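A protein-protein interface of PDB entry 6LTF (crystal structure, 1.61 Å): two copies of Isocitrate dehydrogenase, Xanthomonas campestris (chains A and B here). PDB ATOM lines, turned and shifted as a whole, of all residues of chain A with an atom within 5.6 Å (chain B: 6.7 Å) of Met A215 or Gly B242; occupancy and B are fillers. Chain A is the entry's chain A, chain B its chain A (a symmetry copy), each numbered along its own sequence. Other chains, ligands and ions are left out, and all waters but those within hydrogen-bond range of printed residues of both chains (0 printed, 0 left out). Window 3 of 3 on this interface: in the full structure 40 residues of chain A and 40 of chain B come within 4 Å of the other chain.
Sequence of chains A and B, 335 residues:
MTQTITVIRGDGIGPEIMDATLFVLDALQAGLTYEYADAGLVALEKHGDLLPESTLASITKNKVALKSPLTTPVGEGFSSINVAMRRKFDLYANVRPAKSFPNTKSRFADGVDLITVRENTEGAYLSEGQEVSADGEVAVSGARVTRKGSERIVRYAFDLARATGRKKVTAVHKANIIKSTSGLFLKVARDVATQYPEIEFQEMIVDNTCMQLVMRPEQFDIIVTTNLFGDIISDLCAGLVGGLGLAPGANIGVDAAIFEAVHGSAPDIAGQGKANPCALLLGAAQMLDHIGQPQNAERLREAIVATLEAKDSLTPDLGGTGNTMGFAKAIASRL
1 position is printed for both chains.
Among the printed residues, pairs that only touch across the chains: Met A215 with Gly B242, Val A214 with Gly B239, Met A211 with Gly B239, Met A215 with Gly B239, Val A214 with Leu B240 and Met A211 with Leu B244.
Of the 14 printed residues of chain B, 4 touch a printed residue of chain A. Printed residues of chain B that touch a printed residue of chain A: Gly B239, Leu B240, Gly B242 and Leu B244. Hydrophobic or aromatic side chains of chain B that line the printed part of chain A: Leu B244. Of the 10 printed residues of chain A, 3 touch a printed residue of chain B. Printed residues of chain A that touch a printed residue of chain B: Met A211, Val A214 and Met A215. Among the printed residues, no Asp or Glu carboxylate lies within 4 Å of a Lys or Arg side-chain nitrogen of the other chain.
Of chain B, only Gly B239 and Gly B242 come within 4 Å of Met A215. Of the printed residues of chain A, Gly B242 touches Met A215 (3.2 Å). Printed residues of chain A within 4 Å of Leu B240: Val A214 (3.8 Å). Printed residues of chain B within 4 Å of Met A211: Gly B239 and Leu B244. Of the printed residues of chain A, Gly B239 touches Met A211 (3.6 Å), Val A214 (3.3 Å) and Met A215 (3.6 Å). Printed residues of chain B within 4 Å of Val A214: Gly B239 (3.3 Å) and Leu B240 (3.8 Å). Lys B105 touches none of the printed residues of chain A. The nearest printed residue of chain A that does not touch Gly B242 is Met A211 (6.3 Å). The nearest printed residue of chain A that does not touch Gly B239 is Cys A210 (5.8 Å).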
ATOM      1  N   ARG A 107       5.969 -21.250  17.024  1.00  0.00           N
ATOM      2  CA  ARG A 107       4.533 -21.033  17.148  1.00  0.00           C
ATOM      3  C   ARG A 107       4.114 -21.974  18.269  1.00  0.00           C
ATOM      4  O   ARG A 107       3.410 -22.963  18.037  1.00  0.00           O
ATOM      5  CB  ARG A 107       3.783 -21.286  15.835  1.00  0.00           C
ATOM      6  CG  ARG A 107       2.299 -20.916  15.871  1.00  0.00           C
ATOM      7  CD  ARG A 107       1.398 -22.135  15.732  1.00  0.00           C
ATOM      8  NE  ARG A 107       0.013 -21.856  16.102  1.00  0.00           N
ATOM      9  CZ  ARG A 107      -0.546 -22.298  17.223  1.00  0.00           C
ATOM     10  NH1 ARG A 107       0.173 -23.024  18.067  1.00  0.00           N
ATOM     11  NH2 ARG A 107      -1.814 -22.016  17.505  1.00  0.00           N
ATOM     12  N   CYS A 210      -8.015 -21.727   6.300  1.00  0.00           N
ATOM     13  CA  CYS A 210      -6.719 -21.140   6.638  1.00  0.00           C
ATOM     14  C   CYS A 210      -6.808 -20.267   7.893  1.00  0.00           C
ATOM     15  O   CYS A 210      -5.878 -20.264   8.737  1.00  0.00           O
ATOM     16  CB  CYS A 210      -6.159 -20.368   5.445  1.00  0.00           C
ATOM     17  SG  CYS A 210      -5.743 -21.506   4.069  1.00  0.00           S
ATOM     18  N   MET A 211      -7.934 -19.558   8.062  1.00  0.00           N
ATOM     19  CA  MET A 211      -8.127 -18.802   9.307  1.00  0.00           C
ATOM     20  C   MET A 211      -8.121 -19.732  10.526  1.00  0.00           C
ATOM     21  O   MET A 211      -7.460 -19.462  11.546  1.00  0.00           O
ATOM     22  CB  MET A 211      -9.434 -18.013   9.246  1.00  0.00           C
ATOM     23  CG  MET A 211      -9.548 -16.972  10.359  1.00  0.00           C
ATOM     24  SD  MET A 211     -11.118 -16.076  10.372  1.00  0.00           S
ATOM     25  CE  MET A 211     -12.246 -17.314  10.973  1.00  0.00           C
ATOM     26  N   GLN A 212      -8.867 -20.832  10.435  1.00  0.00           N
ATOM     27  CA  GLN A 212      -8.979 -21.758  11.559  1.00  0.00           C
ATOM     28  C   GLN A 212      -7.649 -22.448  11.846  1.00  0.00           C
ATOM     29  O   GLN A 212      -7.350 -22.786  13.002  1.00  0.00           O
ATOM     30  CB  GLN A 212     -10.069 -22.790  11.261  1.00  0.00           C
ATOM     31  CG  GLN A 212     -11.476 -22.235  11.379  1.00  0.00           C
ATOM     32  CD  GLN A 212     -11.863 -21.790  12.774  1.00  0.00           C
ATOM     33  OE1 GLN A 212     -11.342 -22.277  13.784  1.00  0.00           O
ATOM     34  NE2 GLN A 212     -12.775 -20.832  12.840  1.00  0.00           N
ATOM     35  N   LEU A 213      -6.844 -22.702  10.801  1.00  0.00           N
ATOM     36  CA  LEU A 213      -5.543 -23.331  11.018  1.00  0.00           C
ATOM     37  C   LEU A 213      -4.642 -22.436  11.846  1.00  0.00           C
ATOM     38  O   LEU A 213      -3.839 -22.929  12.647  1.00  0.00           O
ATOM     39  CB  LEU A 213      -4.864 -23.660   9.681  1.00  0.00           C
ATOM     40  CG  LEU A 213      -5.371 -24.943   9.025  1.00  0.00           C
ATOM     41  CD1 LEU A 213      -4.949 -24.934   7.545  1.00  0.00           C
ATOM     42  CD2 LEU A 213      -4.775 -26.173   9.741  1.00  0.00           C
ATOM     43  N   VAL A 214      -4.746 -21.117  11.672  1.00  0.00           N
ATOM     44  CA  VAL A 214      -3.916 -20.296  12.563  1.00  0.00           C
ATOM     45  C   VAL A 214      -4.568 -20.077  13.942  1.00  0.00           C
ATOM     46  O   VAL A 214      -3.862 -19.839  14.928  1.00  0.00           O
ATOM     47  CB  VAL A 214      -3.551 -18.960  11.895  1.00  0.00           C
ATOM     48  CG1 VAL A 214      -2.920 -19.194  10.526  1.00  0.00           C
ATOM     49  CG2 VAL A 214      -4.732 -18.136  11.737  1.00  0.00           C
ATOM     50  N   MET A 215      -5.897 -20.160  14.061  1.00  0.00           N
ATOM     51  CA  MET A 215      -6.505 -19.928  15.377  1.00  0.00           C
ATOM     52  C   MET A 215      -6.527 -21.182  16.245  1.00  0.00           C
ATOM     53  O   MET A 215      -6.371 -21.094  17.471  1.00  0.00           O
ATOM     54  CB  MET A 215      -7.925 -19.388  15.217  1.00  0.00           C
ATOM     55  CG  MET A 215      -7.971 -18.022  14.585  1.00  0.00           C
ATOM     56  SD  MET A 215      -9.653 -17.366  14.437  1.00  0.00           S
ATOM     57  CE  MET A 215     -10.043 -16.995  16.138  1.00  0.00           C
ATOM     58  N   ARG A 216      -6.756 -22.342  15.655  1.00  0.00           N
ATOM     59  CA  ARG A 216      -6.866 -23.573  16.442  1.00  0.00           C
ATOM     60  C   ARG A 216      -6.555 -24.750  15.533  1.00  0.00           C
ATOM     61  O   ARG A 216      -7.465 -25.499  15.131  1.00  0.00           O
ATOM     62  CB  ARG A 216      -8.256 -23.721  17.071  1.00  0.00           C
ATOM     63  CG  ARG A 216      -8.410 -24.955  17.969  1.00  0.00           C
ATOM     64  CD  ARG A 216      -9.671 -24.841  18.830  1.00  0.00           C
ATOM     65  NE  ARG A 216     -10.879 -24.672  18.038  1.00  0.00           N
ATOM     66  CZ  ARG A 216     -11.800 -25.609  17.852  1.00  0.00           C
ATOM     67  NH1 ARG A 216     -11.668 -26.807  18.403  1.00  0.00           N
ATOM     68  NH2 ARG A 216     -12.869 -25.342  17.109  1.00  0.00           N
ATOM     69  N   PRO A 217      -5.276 -24.938  15.200  1.00  0.00           N
ATOM     70  CA  PRO A 217      -4.894 -26.065  14.337  1.00  0.00           C
ATOM     71  C   PRO A 217      -5.173 -27.404  14.978  1.00  0.00           C
ATOM     72  O   PRO A 217      -5.270 -28.416  14.269  1.00  0.00           O
ATOM     73  CB  PRO A 217      -3.390 -25.853  14.113  1.00  0.00           C
ATOM     74  CG  PRO A 217      -2.932 -25.050  15.309  1.00  0.00           C
ATOM     75  CD  PRO A 217      -4.107 -24.153  15.645  1.00  0.00           C
ATOM     76  N   GLU A 218      -5.371 -27.427  16.293  1.00  0.00           N
ATOM     77  CA  GLU A 218      -5.636 -28.672  16.997  1.00  0.00           C
ATOM     78  C   GLU A 218      -6.926 -29.341  16.554  1.00  0.00           C
ATOM     79  O   GLU A 218      -7.083 -30.544  16.790  1.00  0.00           O
ATOM     80  CB  GLU A 218      -5.659 -28.385  18.498  1.00  0.00           C
ATOM     81  CG  GLU A 218      -4.299 -27.901  19.016  1.00  0.00           C
ATOM     82  CD  GLU A 218      -4.158 -26.375  19.067  1.00  0.00           C
ATOM     83  OE1 GLU A 218      -4.946 -25.666  18.397  1.00  0.00           O
ATOM     84  OE2 GLU A 218      -3.257 -25.879  19.788  1.00  0.00           O
ATOM     85  N   THR B 104      -7.457  -8.462  22.772  1.00  0.00           N
ATOM     86  CA  THR B 104      -8.493  -8.726  21.773  1.00  0.00           C
ATOM     87  C   THR B 104      -8.495 -10.178  21.313  1.00  0.00           C
ATOM     88  O   THR B 104      -8.821 -10.456  20.152  1.00  0.00           O
ATOM     89  CB  THR B 104      -8.332  -7.828  20.547  1.00  0.00           C
ATOM     90  OG1 THR B 104      -6.980  -7.904  20.071  1.00  0.00           O
ATOM     91  CG2 THR B 104      -8.688  -6.390  20.867  1.00  0.00           C
ATOM     92  N   LYS B 105      -8.156 -11.110  22.207  1.00  0.00           N
ATOM     93  CA  LYS B 105      -7.801 -12.486  21.853  1.00  0.00           C
ATOM     94  C   LYS B 105      -6.514 -12.454  21.035  1.00  0.00           C
ATOM     95  O   LYS B 105      -5.926 -11.381  20.845  1.00  0.00           O
ATOM     96  CB  LYS B 105      -8.924 -13.225  21.109  1.00  0.00           C
ATOM     97  CG  LYS B 105     -10.350 -12.886  21.553  1.00  0.00           C
ATOM     98  CD  LYS B 105     -10.527 -12.880  23.068  1.00  0.00           C
ATOM     99  CE  LYS B 105     -11.631 -11.908  23.473  1.00  0.00           C
ATOM    100  NZ  LYS B 105     -12.954 -12.287  22.895  1.00  0.00           N
ATOM    101  N   SER B 106      -6.048 -13.603  20.547  1.00  0.00           N
ATOM    102  CA  SER B 106      -4.598 -13.696  20.413  1.00  0.00           C
ATOM    103  C   SER B 106      -4.011 -14.197  19.096  1.00  0.00           C
ATOM    104  O   SER B 106      -4.018 -13.480  18.087  1.00  0.00           O
ATOM    105  CB  SER B 106      -4.069 -14.569  21.553  1.00  0.00           C
ATOM    106  OG  SER B 106      -3.828 -15.902  21.142  1.00  0.00           O
ATOM    107  N   ARG B 107      -3.497 -15.429  19.113  1.00  0.00           N
ATOM    108  CA  ARG B 107      -2.206 -15.704  18.495  1.00  0.00           C
ATOM    109  C   ARG B 107      -1.314 -14.572  18.985  1.00  0.00           C
ATOM    110  O   ARG B 107      -0.906 -13.703  18.206  1.00  0.00           O
ATOM    111  CB  ARG B 107      -2.291 -15.788  16.966  1.00  0.00           C
ATOM    112  CG  ARG B 107      -0.996 -16.235  16.284  1.00  0.00           C
ATOM    113  CD  ARG B 107      -0.388 -15.134  15.426  1.00  0.00           C
ATOM    114  NE  ARG B 107       0.996 -15.414  15.050  1.00  0.00           N
ATOM    115  CZ  ARG B 107       2.037 -14.777  15.573  1.00  0.00           C
ATOM    116  NH1 ARG B 107       1.835 -13.842  16.491  1.00  0.00           N
ATOM    117  NH2 ARG B 107       3.274 -15.071  15.188  1.00  0.00           N
ATOM    118  N   CYS B 237      -4.682 -14.061   7.433  1.00  0.00           N
ATOM    119  CA  CYS B 237      -4.214 -12.936   8.226  1.00  0.00           C
ATOM    120  C   CYS B 237      -5.217 -12.545   9.288  1.00  0.00           C
ATOM    121  O   CYS B 237      -4.822 -12.146  10.384  1.00  0.00           O
ATOM    122  CB  CYS B 237      -3.895 -11.763   7.309  1.00  0.00           C
ATOM    123  SG  CYS B 237      -2.380 -12.052   6.369  1.00  0.00           S
ATOM    124  N   ALA B 238      -6.521 -12.640   8.988  1.00  0.00           N
ATOM    125  CA  ALA B 238      -7.519 -12.394  10.034  1.00  0.00           C
ATOM    126  C   ALA B 238      -7.296 -13.327  11.220  1.00  0.00           C
ATOM    127  O   ALA B 238      -7.444 -12.916  12.386  1.00  0.00           O
ATOM    128  CB  ALA B 238      -8.935 -12.554   9.472  1.00  0.00           C
ATOM    129  N   GLY B 239      -6.943 -14.586  10.944  1.00  0.00           N
ATOM    130  CA  GLY B 239      -6.701 -15.515  12.040  1.00  0.00           C
ATOM    131  C   GLY B 239      -5.502 -15.140  12.892  1.00  0.00           C
ATOM    132  O   GLY B 239      -5.421 -15.523  14.071  1.00  0.00           O
ATOM    133  N   LEU B 240      -4.541 -14.418  12.306  1.00  0.00           N
ATOM    134  CA  LEU B 240      -3.396 -13.967  13.115  1.00  0.00           C
ATOM    135  C   LEU B 240      -3.791 -12.966  14.196  1.00  0.00           C
ATOM    136  O   LEU B 240      -3.103 -12.857  15.219  1.00  0.00           O
ATOM    137  CB  LEU B 240      -2.323 -13.322  12.245  1.00  0.00           C
ATOM    138  CG  LEU B 240      -1.750 -14.165  11.124  1.00  0.00           C
ATOM    139  CD1 LEU B 240      -0.856 -13.301  10.274  1.00  0.00           C
ATOM    140  CD2 LEU B 240      -0.981 -15.348  11.661  1.00  0.00           C
ATOM    141  N   VAL B 241      -4.846 -12.191  13.981  1.00  0.00           N
ATOM    142  CA  VAL B 241      -5.158 -11.088  14.875  1.00  0.00           C
ATOM    143  C   VAL B 241      -6.513 -11.288  15.547  1.00  0.00           C
ATOM    144  O   VAL B 241      -7.194 -10.323  15.884  1.00  0.00           O
ATOM    145  CB  VAL B 241      -5.065  -9.740  14.132  1.00  0.00           C
ATOM    146  CG1 VAL B 241      -3.615  -9.494  13.686  1.00  0.00           C
ATOM    147  CG2 VAL B 241      -5.993  -9.727  12.917  1.00  0.00           C
ATOM    148  N   GLY B 242      -6.916 -12.548  15.714  1.00  0.00           N
ATOM    149  CA  GLY B 242      -8.073 -12.897  16.506  1.00  0.00           C
ATOM    150  C   GLY B 242      -9.302 -13.342  15.749  1.00  0.00           C
ATOM    151  O   GLY B 242     -10.238 -13.852  16.379  1.00  0.00           O
ATOM    152  N   GLY B 243      -9.369 -13.123  14.447  1.00  0.00           N
ATOM    153  CA  GLY B 243     -10.559 -13.472  13.706  1.00  0.00           C
ATOM    154  C   GLY B 243     -11.251 -12.267  13.099  1.00  0.00           C
ATOM    155  O   GLY B 243     -10.707 -11.165  13.029  1.00  0.00           O
ATOM    156  N   LEU B 244     -12.496 -12.492  12.666  1.00  0.00           N
ATOM    157  CA  LEU B 244     -13.263 -11.564  11.840  1.00  0.00           C
ATOM    158  C   LEU B 244     -14.059 -10.536  12.638  1.00  0.00           C
ATOM    159  O   LEU B 244     -14.610  -9.608  12.034  1.00  0.00           O
ATOM    160  CB  LEU B 244     -14.241 -12.337  10.932  1.00  0.00           C
ATOM    161  CG  LEU B 244     -13.649 -13.168   9.794  1.00  0.00           C
ATOM    162  CD1 LEU B 244     -14.750 -13.714   8.895  1.00  0.00           C
ATOM    163  CD2 LEU B 244     -12.644 -12.334   8.992  1.00  0.00           C
ATOM    164  N   GLY B 245     -14.126 -10.663  13.966  1.00  0.00           N
ATOM    165  CA  GLY B 245     -14.969  -9.766  14.745  1.00  0.00           C
ATOM    166  C   GLY B 245     -14.512  -8.320  14.719  1.00  0.00           C
ATOM    167  O   GLY B 245     -15.325  -7.405  14.892  1.00  0.00           O
ATOM    168  N   LEU B 246     -13.213  -8.087  14.515  1.00  0.00           N
ATOM    169  CA  LEU B 246     -12.669  -6.733  14.516  1.00  0.00           C
ATOM    170  C   LEU B 246     -12.148  -6.299  13.148  1.00  0.00           C
ATOM    171  O   LEU B 246     -11.423  -5.302  13.070  1.00  0.00           O
ATOM    172  CB  LEU B 246     -11.546  -6.611  15.549  1.00  0.00           C
ATOM    173  CG  LEU B 246     -11.873  -6.913  17.009  1.00  0.00           C
ATOM    174  CD1 LEU B 246     -10.611  -7.353  17.748  1.00  0.00           C
ATOM    175  CD2 LEU B 246     -12.507  -5.702  17.672  1.00  0.00           C
